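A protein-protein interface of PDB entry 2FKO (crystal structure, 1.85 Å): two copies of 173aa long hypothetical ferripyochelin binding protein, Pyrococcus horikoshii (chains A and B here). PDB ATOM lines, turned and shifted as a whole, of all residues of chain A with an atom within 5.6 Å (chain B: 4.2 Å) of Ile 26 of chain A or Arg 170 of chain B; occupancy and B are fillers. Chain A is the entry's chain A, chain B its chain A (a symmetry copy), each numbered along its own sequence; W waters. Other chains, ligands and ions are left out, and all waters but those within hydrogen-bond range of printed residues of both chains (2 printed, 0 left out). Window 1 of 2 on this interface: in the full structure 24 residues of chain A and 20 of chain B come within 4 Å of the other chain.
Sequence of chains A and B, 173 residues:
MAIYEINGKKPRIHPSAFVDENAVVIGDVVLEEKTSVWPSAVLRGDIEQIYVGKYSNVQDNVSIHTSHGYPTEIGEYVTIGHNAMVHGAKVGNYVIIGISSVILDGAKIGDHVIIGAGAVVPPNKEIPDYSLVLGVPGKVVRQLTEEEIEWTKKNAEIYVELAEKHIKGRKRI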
ATOM      1  N   ALA A   2      12.283  14.136  18.130  1.00  0.00           N
ATOM      2  CA  ALA A   2      12.778  12.925  17.485  1.00  0.00           C
ATOM      3  C   ALA A   2      12.087  13.038  16.148  1.00  0.00           C
ATOM      4  O   ALA A   2      11.164  12.292  15.831  1.00  0.00           O
ATOM      5  CB  ALA A   2      12.338  11.672  18.236  1.00  0.00           C
ATOM      6  N   ILE A   3      12.501  14.108  15.555  1.00  0.00           N
ATOM      7  CA  ILE A   3      11.963  14.373  14.070  1.00  0.00           C
ATOM      8  C   ILE A   3      13.079  14.158  13.051  1.00  0.00           C
ATOM      9  O   ILE A   3      14.216  14.579  13.269  1.00  0.00           O
ATOM     10  CB  ILE A   3      11.391  15.801  13.974  1.00  0.00           C
ATOM     11  CG1 ILE A   3      10.271  15.991  15.004  1.00  0.00           C
ATOM     12  CG2 ILE A   3      10.887  16.083  12.567  1.00  0.00           C
ATOM     13  CD1 ILE A   3      10.347  17.299  15.761  1.00  0.00           C
ATOM     14  N   TYR A   4      12.756  13.507  11.942  1.00  0.00           N
ATOM     15  CA  TYR A   4      13.755  13.235  10.919  1.00  0.00           C
ATOM     16  C   TYR A   4      13.195  13.507   9.540  1.00  0.00           C
ATOM     17  O   TYR A   4      11.983  13.484   9.330  1.00  0.00           O
ATOM     18  CB  TYR A   4      14.176  11.763  10.949  1.00  0.00           C
ATOM     19  CG  TYR A   4      14.605  11.222  12.292  1.00  0.00           C
ATOM     20  CD1 TYR A   4      15.955  11.041  12.596  1.00  0.00           C
ATOM     21  CD2 TYR A   4      13.660  10.863  13.248  1.00  0.00           C
ATOM     22  CE1 TYR A   4      16.350  10.508  13.819  1.00  0.00           C
ATOM     23  CE2 TYR A   4      14.041  10.337  14.469  1.00  0.00           C
ATOM     24  CZ  TYR A   4      15.385  10.158  14.749  1.00  0.00           C
ATOM     25  OH  TYR A   4      15.758   9.616  15.951  1.00  0.00           O
ATOM     26  N   GLU A   5      14.084  13.775   8.594  1.00  0.00           N
ATOM     27  CA  GLU A   5      13.648  13.963   7.220  1.00  0.00           C
ATOM     28  C   GLU A   5      14.229  12.761   6.498  1.00  0.00           C
ATOM     29  O   GLU A   5      15.131  12.097   7.019  1.00  0.00           O
ATOM     30  CB  GLU A   5      14.210  15.252   6.624  1.00  0.00           C
ATOM     31  CG  GLU A   5      15.709  15.402   6.734  1.00  0.00           C
ATOM     32  CD  GLU A   5      16.222  16.558   5.906  1.00  0.00           C
ATOM     33  OE1 GLU A   5      16.896  16.313   4.886  1.00  0.00           O
ATOM     34  OE2 GLU A   5      15.934  17.714   6.270  1.00  0.00           O
ATOM     35  N   ILE A   6      13.697  12.445   5.328  1.00  0.00           N
ATOM     36  CA  ILE A   6      14.237  11.340   4.559  1.00  0.00           C
ATOM     37  C   ILE A   6      14.150  11.693   3.081  1.00  0.00           C
ATOM     38  O   ILE A   6      13.075  11.973   2.557  1.00  0.00           O
ATOM     39  CB  ILE A   6      13.498  10.011   4.857  1.00  0.00           C
ATOM     40  CG1 ILE A   6      14.199   8.867   4.117  1.00  0.00           C
ATOM     41  CG2 ILE A   6      12.025  10.111   4.489  1.00  0.00           C
ATOM     42  CD1 ILE A   6      13.792   7.467   4.585  1.00  0.00           C
ATOM     43  N   ASN A   7      15.306  11.715   2.430  1.00  0.00           N
ATOM     44  CA  ASN A   7      15.403  12.058   1.018  1.00  0.00           C
ATOM     45  C   ASN A   7      14.756  13.405   0.705  1.00  0.00           C
ATOM     46  O   ASN A   7      13.983  13.529  -0.238  1.00  0.00           O
ATOM     47  CB  ASN A   7      14.757  10.971   0.162  1.00  0.00           C
ATOM     48  CG  ASN A   7      15.568   9.695   0.142  1.00  0.00           C
ATOM     49  OD1 ASN A   7      15.193   8.719  -0.501  1.00  0.00           O
ATOM     50  ND2 ASN A   7      16.690   9.700   0.852  1.00  0.00           N
ATOM     51  N   PRO A  11       9.119  16.824   7.867  1.00  0.00           N
ATOM     52  CA  PRO A  11       7.787  16.922   8.461  1.00  0.00           C
ATOM     53  C   PRO A  11       7.419  18.403   8.546  1.00  0.00           C
ATOM     54  O   PRO A  11       8.294  19.268   8.684  1.00  0.00           O
ATOM     55  CB  PRO A  11       7.978  16.305   9.842  1.00  0.00           C
ATOM     56  CG  PRO A  11       9.041  15.282   9.606  1.00  0.00           C
ATOM     57  CD  PRO A  11      10.018  16.016   8.710  1.00  0.00           C
ATOM     58  N   VAL A  24       8.450   9.429  17.413  1.00  0.00           N
ATOM     59  CA  VAL A  24       9.310   9.434  16.232  1.00  0.00           C
ATOM     60  C   VAL A  24       8.507   9.883  15.010  1.00  0.00           C
ATOM     61  O   VAL A  24       7.544   9.230  14.615  1.00  0.00           O
ATOM     62  CB  VAL A  24       9.905   8.026  15.958  1.00  0.00           C
ATOM     63  CG1 VAL A  24      10.661   8.020  14.634  1.00  0.00           C
ATOM     64  CG2 VAL A  24      10.830   7.621  17.096  1.00  0.00           C
ATOM     65  N   VAL A  25       8.902  11.009  14.428  1.00  0.00           N
ATOM     66  CA  VAL A  25       8.218  11.543  13.255  1.00  0.00           C
ATOM     67  C   VAL A  25       9.233  11.577  12.119  1.00  0.00           C
ATOM     68  O   VAL A  25      10.262  12.242  12.213  1.00  0.00           O
ATOM     69  CB  VAL A  25       7.662  12.958  13.540  1.00  0.00           C
ATOM     70  CG1 VAL A  25       6.953  13.505  12.308  1.00  0.00           C
ATOM     71  CG2 VAL A  25       6.687  12.896  14.717  1.00  0.00           C
ATOM     72  N   ILE A  26       8.932  10.850  11.046  1.00  0.00           N
ATOM     73  CA  ILE A  26       9.840  10.741   9.913  1.00  0.00           C
ATOM     74  C   ILE A  26       9.243  11.105   8.554  1.00  0.00           C
ATOM     75  O   ILE A  26       8.151  10.675   8.212  1.00  0.00           O
ATOM     76  CB  ILE A  26      10.373   9.293   9.799  1.00  0.00           C
ATOM     77  CG1 ILE A  26      10.967   8.847  11.137  1.00  0.00           C
ATOM     78  CG2 ILE A  26      11.405   9.202   8.680  1.00  0.00           C
ATOM     79  CD1 ILE A  26      11.197   7.345  11.235  1.00  0.00           C
ATOM     80  N   GLY A  27       9.986  11.898   7.791  1.00  0.00           N
ATOM     81  CA  GLY A  27       9.569  12.270   6.450  1.00  0.00           C
ATOM     82  C   GLY A  27       8.306  13.070   6.167  1.00  0.00           C
ATOM     83  O   GLY A  27       8.010  14.077   6.812  1.00  0.00           O
ATOM     84  N   ASP A  28       7.564  12.599   5.169  1.00  0.00           N
ATOM     85  CA  ASP A  28       6.348  13.256   4.716  1.00  0.00           C
ATOM     86  C   ASP A  28       5.207  13.146   5.724  1.00  0.00           C
ATOM     87  O   ASP A  28       4.307  12.317   5.587  1.00  0.00           O
ATOM     88  CB  ASP A  28       5.940  12.666   3.368  1.00  0.00           C
ATOM     89  CG  ASP A  28       4.951  13.536   2.618  1.00  0.00           C
ATOM     90  OD1 ASP A  28       4.535  13.118   1.518  1.00  0.00           O
ATOM     91  OD2 ASP A  28       4.595  14.626   3.117  1.00  0.00           O
ATOM     92  N   VAL A  29       5.262  14.001   6.739  1.00  0.00           N
ATOM     93  CA  VAL A  29       4.245  14.033   7.777  1.00  0.00           C
ATOM     94  C   VAL A  29       3.832  15.472   8.025  1.00  0.00           C
ATOM     95  O   VAL A  29       4.675  16.356   8.120  1.00  0.00           O
ATOM     96  CB  VAL A  29       4.766  13.441   9.115  1.00  0.00           C
ATOM     97  CG1 VAL A  29       3.669  13.515  10.185  1.00  0.00           C
ATOM     98  CG2 VAL A  29       5.220  11.998   8.910  1.00  0.00           C
ATOM     99  N   VAL A  42       4.837   6.487  16.708  1.00  0.00           N
ATOM    100  CA  VAL A  42       5.651   6.550  15.505  1.00  0.00           C
ATOM    101  C   VAL A  42       4.836   6.874  14.266  1.00  0.00           C
ATOM    102  O   VAL A  42       3.870   6.183  13.951  1.00  0.00           O
ATOM    103  CB  VAL A  42       6.378   5.204  15.251  1.00  0.00           C
ATOM    104  CG1 VAL A  42       7.212   5.290  13.968  1.00  0.00           C
ATOM    105  CG2 VAL A  42       7.261   4.852  16.442  1.00  0.00           C
ATOM    106  N   LEU A  43       5.228   7.943  13.577  1.00  0.00           N
ATOM    107  CA  LEU A  43       4.570   8.356  12.346  1.00  0.00           C
ATOM    108  C   LEU A  43       5.643   8.273  11.268  1.00  0.00           C
ATOM    109  O   LEU A  43       6.455   9.186  11.113  1.00  0.00           O
ATOM    110  CB  LEU A  43       4.028   9.785  12.466  1.00  0.00           C
ATOM    111  CG  LEU A  43       2.851   9.955  13.436  1.00  0.00           C
ATOM    112  CD1 LEU A  43       3.354   9.844  14.865  1.00  0.00           C
ATOM    113  CD2 LEU A  43       2.189  11.307  13.218  1.00  0.00           C
ATOM    114  N   ARG A  44       5.646   7.166  10.534  1.00  0.00           N
ATOM    115  CA  ARG A  44       6.650   6.940   9.502  1.00  0.00           C
ATOM    116  C   ARG A  44       6.178   7.318   8.101  1.00  0.00           C
ATOM    117  O   ARG A  44       5.533   6.535   7.407  1.00  0.00           O
ATOM    118  CB  ARG A  44       7.109   5.475   9.556  1.00  0.00           C
ATOM    119  CG  ARG A  44       8.331   5.143   8.698  1.00  0.00           C
ATOM    120  CD  ARG A  44       9.259   4.140   9.402  1.00  0.00           C
ATOM    121  NE  ARG A  44       8.629   2.849   9.692  1.00  0.00           N
ATOM    122  CZ  ARG A  44       8.409   1.894   8.790  1.00  0.00           C
ATOM    123  NH1 ARG A  44       8.764   2.070   7.527  1.00  0.00           N
ATOM    124  NH2 ARG A  44       7.835   0.752   9.157  1.00  0.00           N
ATOM    125  N   GLY A  45       6.515   8.535   7.694  1.00  0.00           N
ATOM    126  CA  GLY A  45       6.119   9.013   6.382  1.00  0.00           C
ATOM    127  C   GLY A  45       7.201   8.762   5.357  1.00  0.00           C
ATOM    128  O   GLY A  45       7.661   9.692   4.701  1.00  0.00           O
ATOM    129  N   ASP A  46       7.601   7.502   5.210  1.00  0.00           N
ATOM    130  CA  ASP A  46       8.650   7.146   4.266  1.00  0.00           C
ATOM    131  C   ASP A  46       8.147   6.567   2.949  1.00  0.00           C
ATOM    132  O   ASP A  46       8.941   6.262   2.068  1.00  0.00           O
ATOM    133  CB  ASP A  46       9.645   6.181   4.922  1.00  0.00           C
ATOM    134  CG  ASP A  46       8.983   4.921   5.454  1.00  0.00           C
ATOM    135  OD1 ASP A  46       7.744   4.786   5.325  1.00  0.00           O
ATOM    136  OD2 ASP A  46       9.708   4.066   6.003  1.00  0.00           O
ATOM    137  N   PHE B  18      19.632  -2.566   9.047  1.00  0.00           N
ATOM    138  CA  PHE B  18      19.290  -1.223   9.484  1.00  0.00           C
ATOM    139  C   PHE B  18      18.594  -1.329  10.825  1.00  0.00           C
ATOM    140  O   PHE B  18      17.558  -1.981  10.947  1.00  0.00           O
ATOM    141  CB  PHE B  18      18.343  -0.517   8.512  1.00  0.00           C
ATOM    142  CG  PHE B  18      17.756   0.759   9.075  1.00  0.00           C
ATOM    143  CD1 PHE B  18      18.577   1.847   9.368  1.00  0.00           C
ATOM    144  CD2 PHE B  18      16.392   0.857   9.349  1.00  0.00           C
ATOM    145  CE1 PHE B  18      18.048   3.017   9.928  1.00  0.00           C
ATOM    146  CE2 PHE B  18      15.856   2.023   9.907  1.00  0.00           C
ATOM    147  CZ  PHE B  18      16.687   3.104  10.197  1.00  0.00           C
ATOM    148  N   ASP B  20      17.042   1.142  13.515  1.00  0.00           N
ATOM    149  CA  ASP B  20      16.683   2.516  13.819  1.00  0.00           C
ATOM    150  C   ASP B  20      17.272   2.872  15.182  1.00  0.00           C
ATOM    151  O   ASP B  20      17.287   2.040  16.084  1.00  0.00           O
ATOM    152  CB  ASP B  20      15.165   2.655  13.860  1.00  0.00           C
ATOM    153  CG  ASP B  20      14.722   4.091  13.904  1.00  0.00           C
ATOM    154  OD1 ASP B  20      14.539   4.686  12.818  1.00  0.00           O
ATOM    155  OD2 ASP B  20      14.570   4.626  15.028  1.00  0.00           O
ATOM    156  N   PRO B  39      11.619   1.963  14.398  1.00  0.00           N
ATOM    157  CA  PRO B  39      11.339   2.746  15.603  1.00  0.00           C
ATOM    158  C   PRO B  39      10.511   2.042  16.672  1.00  0.00           C
ATOM    159  O   PRO B  39       9.452   1.487  16.391  1.00  0.00           O
ATOM    160  CB  PRO B  39      10.643   3.986  15.053  1.00  0.00           C
ATOM    161  CG  PRO B  39      11.331   4.183  13.749  1.00  0.00           C
ATOM    162  CD  PRO B  39      11.393   2.779  13.191  1.00  0.00           C
ATOM    163  N   LYS B 165      16.840   2.915   1.941  1.00  0.00           N
ATOM    164  CA  LYS B 165      16.501   4.327   1.824  1.00  0.00           C
ATOM    165  C   LYS B 165      16.831   5.066   3.117  1.00  0.00           C
ATOM    166  O   LYS B 165      17.362   6.176   3.092  1.00  0.00           O
ATOM    167  CB  LYS B 165      15.019   4.499   1.476  1.00  0.00           C
ATOM    168  CG  LYS B 165      14.603   3.830   0.173  1.00  0.00           C
ATOM    169  CD  LYS B 165      13.117   4.019  -0.104  1.00  0.00           C
ATOM    170  CE  LYS B 165      12.709   3.348  -1.408  1.00  0.00           C
ATOM    171  NZ  LYS B 165      11.258   3.522  -1.694  1.00  0.00           N
ATOM    172  N   HIS B 166      16.497   4.428   4.238  1.00  0.00           N
ATOM    173  CA  HIS B 166      16.748   5.023   5.543  1.00  0.00           C
ATOM    174  C   HIS B 166      18.235   5.102   5.872  1.00  0.00           C
ATOM    175  O   HIS B 166      18.713   6.111   6.393  1.00  0.00           O
ATOM    176  CB  HIS B 166      16.003   4.232   6.624  1.00  0.00           C
ATOM    177  CG  HIS B 166      14.535   4.530   6.675  1.00  0.00           C
ATOM    178  ND1 HIS B 166      13.970   5.318   7.656  1.00  0.00           N
ATOM    179  CD2 HIS B 166      13.521   4.168   5.855  1.00  0.00           C
ATOM    180  CE1 HIS B 166      12.672   5.425   7.440  1.00  0.00           C
ATOM    181  NE2 HIS B 166      12.372   4.737   6.353  1.00  0.00           N
ATOM    182  N   LYS B 168      20.689   5.410   3.879  1.00  0.00           N
ATOM    183  CA  LYS B 168      21.316   6.457   3.080  1.00  0.00           C
ATOM    184  C   LYS B 168      20.733   7.864   3.185  1.00  0.00           C
ATOM    185  O   LYS B 168      21.468   8.841   3.039  1.00  0.00           O
ATOM    186  CB  LYS B 168      21.323   6.046   1.606  1.00  0.00           C
ATOM    187  CG  LYS B 168      22.042   4.740   1.341  1.00  0.00           C
ATOM    188  CD  LYS B 168      22.024   4.379  -0.129  1.00  0.00           C
ATOM    189  CE  LYS B 168      22.638   3.004  -0.341  1.00  0.00           C
ATOM    190  NZ  LYS B 168      22.784   2.664  -1.779  1.00  0.00           N
ATOM    191  N   GLY B 169      19.431   7.975   3.448  1.00  0.00           N
ATOM    192  CA  GLY B 169      18.813   9.287   3.488  1.00  0.00           C
ATOM    193  C   GLY B 169      18.188   9.845   4.751  1.00  0.00           C
ATOM    194  O   GLY B 169      17.612  10.932   4.703  1.00  0.00           O
ATOM    195  N   ARG B 170      18.271   9.129   5.869  1.00  0.00           N
ATOM    196  CA  ARG B 170      17.691   9.625   7.117  1.00  0.00           C
ATOM    197  C   ARG B 170      18.570  10.712   7.705  1.00  0.00           C
ATOM    198  O   ARG B 170      19.798  10.627   7.657  1.00  0.00           O
ATOM    199  CB  ARG B 170      17.550   8.500   8.144  1.00  0.00           C
ATOM    200  CG  ARG B 170      16.252   7.707   8.051  1.00  0.00           C
ATOM    201  CD  ARG B 170      15.100   8.414   8.759  1.00  0.00           C
ATOM    202  NE  ARG B 170      15.175   8.322  10.215  1.00  0.00           N
ATOM    203  CZ  ARG B 170      14.929   7.218  10.917  1.00  0.00           C
ATOM    204  NH1 ARG B 170      14.589   6.091  10.307  1.00  0.00           N
ATOM    205  NH2 ARG B 170      15.013   7.244  12.240  1.00  0.00           N
ATOM    206  N   LYS B 171      17.931  11.736   8.256  1.00  0.00           N
ATOM    207  CA  LYS B 171      18.640  12.841   8.880  1.00  0.00           C
ATOM    208  C   LYS B 171      17.816  13.426  10.014  1.00  0.00           C
ATOM    209  O   LYS B 171      16.675  13.833   9.817  1.00  0.00           O
ATOM    210  CB  LYS B 171      18.938  13.943   7.865  1.00  0.00           C
ATOM    211  CG  LYS B 171      20.175  13.702   7.012  1.00  0.00           C
ATOM    212  CD  LYS B 171      20.493  14.921   6.150  1.00  0.00           C
ATOM    213  CE  LYS B 171      20.765  16.155   7.010  1.00  0.00           C
ATOM    214  NZ  LYS B 171      20.995  17.400   6.219  1.00  0.00           N
HETATM  215  O   HOH W   1      18.187  13.380   3.716  1.00  0.00           O
HETATM  216  O   HOH W   2       9.352   5.402  -0.571  1.00  0.00           O
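The backbone carbonyl oxygen of Val 25 of chain A is in hydrogen-bond range of the backbone NH of Tyr 4 of chain A (2.8 Å). The backbone NH (N) of Gly 27 of chain A sits at hydrogen-bond distance from the backbone carbonyl oxygen (O) of Tyr 4 of chain A. The backbone NH (N) of Ile 26 of chain A is in hydrogen-bond range of the backbone carbonyl oxygen (O) of Leu 43 of chain A (3.0 Å). N of Gly 45 of chain A is in hydrogen-bond range of O of Ile 26 of chain A, at 2.7 Å. The guanidinium group of Arg 44 of chain A lies within salt-bridge range of the side-chain carboxylate of Asp 46 of chain A, at 2.7 Å. ND1 of His 166 of chain B sits at hydrogen-bond distance from NH1 of Arg 170 of chain B (2.8 Å).
CG of Tyr 4 of chain A touches NE of Arg 170 of chain B (3.6 Å). Lys 171 of chain B touches Tyr 4 of chain A (O to CA, 3.2 Å). Glu 5 of chain A touches Gly 169 of chain B. CA of Arg 170 of chain B touches O of Glu 5 of chain A, 3.6 Å away. CD1 of Ile 6 of chain A touches CD2 of His 166 of chain B, at 3.5 Å. Gly 169 of chain B touches Ile 6 of chain A. Pro 39 of chain B touches Val 24 of chain A (CG to CG1, 3.99 Å). Ile 26 of chain A touches Arg 170 of chain B (CD1 to NH1, 3.7 Å). Val 42 of chain A touches Pro 39 of chain B (CG2 to CB, 3.8 Å).
Ile 26 of chain A touches one residue of chain B. Arg 170 of chain B touches just these residues of chain A: Tyr 4 (3.6 Å), Glu 5 (3.6 Å) and Ile 26 (3.7 Å). Of the printed residues of chain A, Lys 171 of chain B touches Tyr 4 (3.2 Å) and Glu 5 (2.9 Å). Of the printed residues of chain B, Tyr 4 of chain A touches Arg 170 (3.6 Å) and Lys 171 (3.2 Å). Of the printed residues of chain B, Val 24 of chain A touches Pro 39 (3.99 Å). Of the printed residues of chain B, Asp 46 of chain A touches His 166 (2.8 Å). Of the printed residues of chain A, Gly 169 of chain B touches Glu 5 (3.6 Å), Ile 6 (3.4 Å) and Asn 7 (3.3 Å). Ala 2 of chain A touches none of the printed residues of chain B. Pro 11 of chain A touches none of the printed residues of chain B. The nearest printed residue of chain B that does not touch Asp 46 of chain A is Lys 165 of chain B (5.2 Å).
N of Glu 5 of chain A sits at hydrogen-bond distance from O of Lys 171 of chain B (2.9 Å). O of Gly 169 of chain B sits at hydrogen-bond distance from N of Asn 7 of chain A, at 3.3 Å. The side-chain carboxylate of Asp 46 of chain A lies within hydrogen-bond range of a ring nitrogen (NE2) of His 166 of chain B (2.8 Å).
Of the 18 printed residues of chain A, 8 touch a printed residue of chain B. Among the printed residues, no Asp or Glu carboxylate lies within 4 Å of a Lys or Arg side-chain nitrogen of the other chain.
No position is printed for both chains. Of the 12 pairs that touch across the chains among the printed residues, none has its exchanged pair printed and touching as well.
Water W1 lies within hydrogen-bond range of O of Gly 169 of chain B (2.7 Å) and OE1 of Glu 5 of chain A (3.4 Å). Water W2 bridges O of Asp 46 of chain A (2.8 Å) and NZ of Lys 165 of chain B (2.9 Å).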
